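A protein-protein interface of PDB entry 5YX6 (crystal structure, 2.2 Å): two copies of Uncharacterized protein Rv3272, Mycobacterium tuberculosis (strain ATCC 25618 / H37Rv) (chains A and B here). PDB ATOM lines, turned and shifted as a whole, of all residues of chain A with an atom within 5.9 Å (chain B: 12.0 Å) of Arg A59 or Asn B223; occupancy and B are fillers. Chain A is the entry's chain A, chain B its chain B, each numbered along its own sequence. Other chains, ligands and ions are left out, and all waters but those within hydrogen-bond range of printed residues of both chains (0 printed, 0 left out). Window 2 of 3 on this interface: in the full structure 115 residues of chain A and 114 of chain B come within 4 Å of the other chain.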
ATOM      1  N   VAL A  55      17.506 -22.091 -32.061  1.00  0.00           N
ATOM      2  CA  VAL A  55      18.193 -23.028 -31.165  1.00  0.00           C
ATOM      3  C   VAL A  55      18.060 -22.702 -29.671  1.00  0.00           C
ATOM      4  O   VAL A  55      18.363 -21.591 -29.236  1.00  0.00           O
ATOM      5  CB  VAL A  55      19.701 -23.106 -31.502  1.00  0.00           C
ATOM      6  CG1 VAL A  55      20.462 -23.808 -30.387  1.00  0.00           C
ATOM      7  CG2 VAL A  55      19.914 -23.820 -32.833  1.00  0.00           C
ATOM      8  N   LEU A  56      17.613 -23.689 -28.898  1.00  0.00           N
ATOM      9  CA  LEU A  56      17.595 -23.611 -27.440  1.00  0.00           C
ATOM     10  C   LEU A  56      18.514 -24.673 -26.866  1.00  0.00           C
ATOM     11  O   LEU A  56      18.165 -25.851 -26.892  1.00  0.00           O
ATOM     12  CB  LEU A  56      16.182 -23.823 -26.890  1.00  0.00           C
ATOM     13  CG  LEU A  56      15.073 -22.811 -27.166  1.00  0.00           C
ATOM     14  CD1 LEU A  56      13.775 -23.279 -26.527  1.00  0.00           C
ATOM     15  CD2 LEU A  56      15.475 -21.447 -26.640  1.00  0.00           C
ATOM     16  N   PRO A  57      19.689 -24.273 -26.352  1.00  0.00           N
ATOM     17  CA  PRO A  57      20.681 -25.213 -25.804  1.00  0.00           C
ATOM     18  C   PRO A  57      20.095 -26.233 -24.817  1.00  0.00           C
ATOM     19  O   PRO A  57      19.555 -25.838 -23.776  1.00  0.00           O
ATOM     20  CB  PRO A  57      21.678 -24.291 -25.100  1.00  0.00           C
ATOM     21  CG  PRO A  57      21.615 -23.032 -25.881  1.00  0.00           C
ATOM     22  CD  PRO A  57      20.179 -22.885 -26.332  1.00  0.00           C
ATOM     23  N   GLY A  58      20.204 -27.514 -25.195  1.00  0.00           N
ATOM     24  CA  GLY A  58      19.763 -28.711 -24.451  1.00  0.00           C
ATOM     25  C   GLY A  58      18.292 -29.084 -24.665  1.00  0.00           C
ATOM     26  O   GLY A  58      17.803 -30.051 -24.075  1.00  0.00           O
ATOM     27  N   ARG A  59      17.590 -28.335 -25.509  1.00  0.00           N
ATOM     28  CA  ARG A  59      16.153 -28.529 -25.680  1.00  0.00           C
ATOM     29  C   ARG A  59      15.766 -28.526 -27.153  1.00  0.00           C
ATOM     30  O   ARG A  59      16.512 -28.012 -27.986  1.00  0.00           O
ATOM     31  CB  ARG A  59      15.382 -27.441 -24.927  1.00  0.00           C
ATOM     32  CG  ARG A  59      15.578 -27.476 -23.419  1.00  0.00           C
ATOM     33  CD  ARG A  59      15.390 -26.104 -22.799  1.00  0.00           C
ATOM     34  NE  ARG A  59      14.038 -25.598 -23.000  1.00  0.00           N
ATOM     35  CZ  ARG A  59      13.603 -24.434 -22.533  1.00  0.00           C
ATOM     36  NH1 ARG A  59      12.354 -24.052 -22.761  1.00  0.00           N
ATOM     37  NH2 ARG A  59      14.418 -23.653 -21.837  1.00  0.00           N
ATOM     38  N   PRO A  60      14.601 -29.115 -27.483  1.00  0.00           N
ATOM     39  CA  PRO A  60      14.106 -29.000 -28.861  1.00  0.00           C
ATOM     40  C   PRO A  60      13.990 -27.533 -29.294  1.00  0.00           C
ATOM     41  O   PRO A  60      13.589 -26.682 -28.484  1.00  0.00           O
ATOM     42  CB  PRO A  60      12.727 -29.669 -28.800  1.00  0.00           C
ATOM     43  CG  PRO A  60      12.806 -30.607 -27.638  1.00  0.00           C
ATOM     44  CD  PRO A  60      13.719 -29.949 -26.642  1.00  0.00           C
ATOM     45  N   PRO A  61      14.364 -27.242 -30.551  1.00  0.00           N
ATOM     46  CA  PRO A  61      14.264 -25.914 -31.169  1.00  0.00           C
ATOM     47  C   PRO A  61      12.891 -25.245 -30.973  1.00  0.00           C
ATOM     48  O   PRO A  61      11.864 -25.925 -30.861  1.00  0.00           O
ATOM     49  CB  PRO A  61      14.519 -26.212 -32.650  1.00  0.00           C
ATOM     50  CG  PRO A  61      15.407 -27.401 -32.639  1.00  0.00           C
ATOM     51  CD  PRO A  61      14.965 -28.231 -31.467  1.00  0.00           C
ATOM     52  N   LEU A  62      12.891 -23.915 -30.941  1.00  0.00           N
ATOM     53  CA  LEU A  62      11.680 -23.133 -30.724  1.00  0.00           C
ATOM     54  C   LEU A  62      11.188 -22.456 -32.006  1.00  0.00           C
ATOM     55  O   LEU A  62      11.880 -21.616 -32.587  1.00  0.00           O
ATOM     56  CB  LEU A  62      11.922 -22.091 -29.625  1.00  0.00           C
ATOM     57  CG  LEU A  62      10.921 -20.951 -29.398  1.00  0.00           C
ATOM     58  CD1 LEU A  62       9.478 -21.454 -29.333  1.00  0.00           C
ATOM     59  CD2 LEU A  62      11.286 -20.205 -28.125  1.00  0.00           C
ATOM     60  N   THR A 359       8.807 -26.407 -21.016  1.00  0.00           N
ATOM     61  CA  THR A 359       7.839 -25.323 -21.178  1.00  0.00           C
ATOM     62  C   THR A 359       8.499 -24.080 -21.828  1.00  0.00           C
ATOM     63  O   THR A 359       9.716 -23.909 -21.764  1.00  0.00           O
ATOM     64  CB  THR A 359       7.206 -24.965 -19.804  1.00  0.00           C
ATOM     65  OG1 THR A 359       5.777 -24.924 -19.913  1.00  0.00           O
ATOM     66  CG2 THR A 359       7.719 -23.629 -19.284  1.00  0.00           C
ATOM     67  N   ILE A 360       7.691 -23.242 -22.479  1.00  0.00           N
ATOM     68  CA  ILE A 360       8.166 -22.051 -23.195  1.00  0.00           C
ATOM     69  C   ILE A 360       7.467 -20.740 -22.806  1.00  0.00           C
ATOM     70  O   ILE A 360       6.263 -20.722 -22.558  1.00  0.00           O
ATOM     71  CB  ILE A 360       8.056 -22.289 -24.725  1.00  0.00           C
ATOM     72  CG1 ILE A 360       9.149 -23.277 -25.141  1.00  0.00           C
ATOM     73  CG2 ILE A 360       8.238 -21.012 -25.521  1.00  0.00           C
ATOM     74  CD1 ILE A 360       9.127 -23.657 -26.594  1.00  0.00           C
ATOM     75  N   THR A 361       8.230 -19.648 -22.744  1.00  0.00           N
ATOM     76  CA  THR A 361       7.713 -18.339 -22.331  1.00  0.00           C
ATOM     77  C   THR A 361       7.372 -17.430 -23.516  1.00  0.00           C
ATOM     78  O   THR A 361       8.204 -17.202 -24.388  1.00  0.00           O
ATOM     79  CB  THR A 361       8.731 -17.621 -21.432  1.00  0.00           C
ATOM     80  OG1 THR A 361       9.030 -18.451 -20.304  1.00  0.00           O
ATOM     81  CG2 THR A 361       8.180 -16.294 -20.947  1.00  0.00           C
ATOM     82  N   VAL A 362       6.150 -16.903 -23.553  1.00  0.00           N
ATOM     83  CA  VAL A 362       5.795 -15.959 -24.608  1.00  0.00           C
ATOM     84  C   VAL A 362       5.147 -14.704 -24.028  1.00  0.00           C
ATOM     85  O   VAL A 362       4.803 -14.661 -22.844  1.00  0.00           O
ATOM     86  CB  VAL A 362       4.845 -16.595 -25.668  1.00  0.00           C
ATOM     87  CG1 VAL A 362       5.455 -17.862 -26.252  1.00  0.00           C
ATOM     88  CG2 VAL A 362       3.461 -16.881 -25.086  1.00  0.00           C
ATOM     89  N   GLN B 214       7.730  -5.666 -30.333  1.00  0.00           N
ATOM     90  CA  GLN B 214       9.067  -6.255 -30.348  1.00  0.00           C
ATOM     91  C   GLN B 214       9.060  -7.684 -29.817  1.00  0.00           C
ATOM     92  O   GLN B 214      10.095  -8.189 -29.387  1.00  0.00           O
ATOM     93  CB  GLN B 214      10.044  -5.423 -29.502  1.00  0.00           C
ATOM     94  CG  GLN B 214      10.009  -3.918 -29.727  1.00  0.00           C
ATOM     95  CD  GLN B 214      10.729  -3.146 -28.615  1.00  0.00           C
ATOM     96  OE1 GLN B 214      11.945  -2.913 -28.672  1.00  0.00           O
ATOM     97  NE2 GLN B 214       9.970  -2.742 -27.600  1.00  0.00           N
ATOM     98  N   ALA B 215       7.900  -8.327 -29.829  1.00  0.00           N
ATOM     99  CA  ALA B 215       7.727  -9.579 -29.090  1.00  0.00           C
ATOM    100  C   ALA B 215       8.757 -10.685 -29.422  1.00  0.00           C
ATOM    101  O   ALA B 215       9.309 -11.294 -28.507  1.00  0.00           O
ATOM    102  CB  ALA B 215       6.313 -10.094 -29.290  1.00  0.00           C
ATOM    103  N   ASN B 216       9.025 -10.948 -30.701  1.00  0.00           N
ATOM    104  CA  ASN B 216      10.004 -11.987 -31.054  1.00  0.00           C
ATOM    105  C   ASN B 216      11.424 -11.684 -30.557  1.00  0.00           C
ATOM    106  O   ASN B 216      12.149 -12.589 -30.136  1.00  0.00           O
ATOM    107  CB  ASN B 216      10.014 -12.252 -32.569  1.00  0.00           C
ATOM    108  CG  ASN B 216       8.690 -12.841 -33.066  1.00  0.00           C
ATOM    109  OD1 ASN B 216       8.116 -13.725 -32.419  1.00  0.00           O
ATOM    110  ND2 ASN B 216       8.211 -12.369 -34.218  1.00  0.00           N
ATOM    111  N   GLN B 217      11.812 -10.416 -30.592  1.00  0.00           N
ATOM    112  CA  GLN B 217      13.133 -10.033 -30.121  1.00  0.00           C
ATOM    113  C   GLN B 217      13.242 -10.181 -28.604  1.00  0.00           C
ATOM    114  O   GLN B 217      14.294 -10.560 -28.099  1.00  0.00           O
ATOM    115  CB  GLN B 217      13.454  -8.596 -30.521  1.00  0.00           C
ATOM    116  CG  GLN B 217      13.737  -8.415 -32.003  1.00  0.00           C
ATOM    117  CD  GLN B 217      12.483  -8.593 -32.838  1.00  0.00           C
ATOM    118  OE1 GLN B 217      11.385  -8.253 -32.393  1.00  0.00           O
ATOM    119  NE2 GLN B 217      12.635  -9.114 -34.051  1.00  0.00           N
ATOM    120  N   LEU B 218      12.173  -9.859 -27.877  1.00  0.00           N
ATOM    121  CA  LEU B 218      12.161 -10.002 -26.419  1.00  0.00           C
ATOM    122  C   LEU B 218      12.154 -11.465 -26.015  1.00  0.00           C
ATOM    123  O   LEU B 218      12.699 -11.849 -24.988  1.00  0.00           O
ATOM    124  CB  LEU B 218      10.938  -9.318 -25.807  1.00  0.00           C
ATOM    125  CG  LEU B 218      10.974  -7.866 -25.338  1.00  0.00           C
ATOM    126  CD1 LEU B 218      12.378  -7.306 -25.367  1.00  0.00           C
ATOM    127  CD2 LEU B 218      10.004  -7.009 -26.143  1.00  0.00           C
ATOM    128  N   MET B 219      11.506 -12.273 -26.839  1.00  0.00           N
ATOM    129  CA  MET B 219      11.227 -13.663 -26.510  1.00  0.00           C
ATOM    130  C   MET B 219      12.481 -14.523 -26.441  1.00  0.00           C
ATOM    131  O   MET B 219      12.533 -15.500 -25.701  1.00  0.00           O
ATOM    132  CB  MET B 219      10.259 -14.234 -27.536  1.00  0.00           C
ATOM    133  CG  MET B 219       9.435 -15.381 -27.041  1.00  0.00           C
ATOM    134  SD  MET B 219       8.379 -15.919 -28.376  1.00  0.00           S
ATOM    135  CE  MET B 219       9.573 -16.486 -29.591  1.00  0.00           C
ATOM    136  N   MET B 220      13.484 -14.162 -27.227  1.00  0.00           N
ATOM    137  CA  MET B 220      14.746 -14.882 -27.212  1.00  0.00           C
ATOM    138  C   MET B 220      15.447 -14.801 -25.856  1.00  0.00           C
ATOM    139  O   MET B 220      16.143 -15.733 -25.454  1.00  0.00           O
ATOM    140  CB  MET B 220      15.657 -14.353 -28.315  1.00  0.00           C
ATOM    141  CG  MET B 220      15.184 -14.726 -29.713  1.00  0.00           C
ATOM    142  SD  MET B 220      14.932 -16.509 -29.918  1.00  0.00           S
ATOM    143  CE  MET B 220      13.139 -16.623 -29.858  1.00  0.00           C
ATOM    144  N   HIS B 221      15.248 -13.700 -25.139  1.00  0.00           N
ATOM    145  CA  HIS B 221      15.869 -13.552 -23.828  1.00  0.00           C
ATOM    146  C   HIS B 221      15.002 -14.106 -22.702  1.00  0.00           C
ATOM    147  O   HIS B 221      15.458 -14.229 -21.566  1.00  0.00           O
ATOM    148  CB  HIS B 221      16.210 -12.087 -23.563  1.00  0.00           C
ATOM    149  CG  HIS B 221      17.091 -11.486 -24.611  1.00  0.00           C
ATOM    150  ND1 HIS B 221      18.441 -11.753 -24.687  1.00  0.00           N
ATOM    151  CD2 HIS B 221      16.819 -10.625 -25.619  1.00  0.00           C
ATOM    152  CE1 HIS B 221      18.960 -11.089 -25.705  1.00  0.00           C
ATOM    153  NE2 HIS B 221      17.997 -10.396 -26.285  1.00  0.00           N
ATOM    154  N   LEU B 222      13.755 -14.442 -23.008  1.00  0.00           N
ATOM    155  CA  LEU B 222      12.892 -15.065 -22.013  1.00  0.00           C
ATOM    156  C   LEU B 222      13.093 -16.580 -21.979  1.00  0.00           C
ATOM    157  O   LEU B 222      12.672 -17.245 -21.029  1.00  0.00           O
ATOM    158  CB  LEU B 222      11.424 -14.738 -22.291  1.00  0.00           C
ATOM    159  CG  LEU B 222      10.974 -13.291 -22.070  1.00  0.00           C
ATOM    160  CD1 LEU B 222       9.557 -13.104 -22.579  1.00  0.00           C
ATOM    161  CD2 LEU B 222      11.088 -12.883 -20.597  1.00  0.00           C
ATOM    162  N   ASN B 223      13.766 -17.117 -22.995  1.00  0.00           N
ATOM    163  CA  ASN B 223      13.924 -18.566 -23.130  1.00  0.00           C
ATOM    164  C   ASN B 223      15.379 -19.053 -23.252  1.00  0.00           C
ATOM    165  O   ASN B 223      15.765 -20.018 -22.595  1.00  0.00           O
ATOM    166  CB  ASN B 223      13.124 -19.059 -24.348  1.00  0.00           C
ATOM    167  CG  ASN B 223      11.616 -18.878 -24.185  1.00  0.00           C
ATOM    168  OD1 ASN B 223      10.951 -19.667 -23.512  1.00  0.00           O
ATOM    169  ND2 ASN B 223      11.074 -17.836 -24.807  1.00  0.00           N
ATOM    170  N   ARG B 224      16.181 -18.396 -24.089  1.00  0.00           N
ATOM    171  CA  ARG B 224      17.550 -18.851 -24.347  1.00  0.00           C
ATOM    172  C   ARG B 224      18.497 -18.170 -23.376  1.00  0.00           C
ATOM    173  O   ARG B 224      18.224 -18.137 -22.180  1.00  0.00           O
ATOM    174  CB  ARG B 224      17.973 -18.569 -25.796  1.00  0.00           C
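The backbone NH of Thr A361 is in hydrogen-bond range of the side-chain amide oxygen of Asn B223 (2.8 Å).
Among the printed residues, merely in contact across the chains: Leu A56 with Arg B224 (3.9 Å), Arg A59 with Asn B223 (3.9 Å), Ile A360 with Asn B223 (3.6 Å), Thr A361 with Met B219 (3.4 Å) and Thr A361 with Leu B222 (3.8 Å).
No position is printed for both chains.
Of the 11 printed residues of chain B, 4 touch a printed residue of chain A.
Hydrophobic or aromatic side chains of chain B within 4 Å of the printed part of chain A: Met B219 and Leu B222.
Among the printed residues, no Asp or Glu carboxylate lies within 4 Å of a Lys or Arg side-chain nitrogen of the other chain.
Printed residues of chain B within 4 Å of Arg A59: Asn B223.
No residue of chain B comes within 4 Å of Val A55.
No residue of chain B comes within 4 Å of Gly A58.
No residue of chain B comes within 4 Å of Pro A60.
No residue of chain B comes within 4 Å of Val A362.
Printed residues of chain A within 4 Å of Arg B224: Leu A56.
Of the printed residues of chain A, Leu B222 touches Thr A361.
Of the printed residues of chain A, Met B219 touches Thr A361.
His B221 touches none of the printed residues of chain A.
Ala B215 touches none of the printed residues of chain A.
The nearest residue of chain B that does not touch Arg A59 is Arg B224 (6.0 Å).
The nearest printed residue of chain A that does not touch Asn B223 is Leu A56 (4.1 Å).
The backbone carbonyl oxygen (O) of Thr A359 lies within hydrogen-bond range of the guanidinium group (NH1) of Arg A59.
The backbone carbonyl oxygen of Met B219 sits at hydrogen-bond distance from the side-chain amide nitrogen of Asn B223 (2.9 Å).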
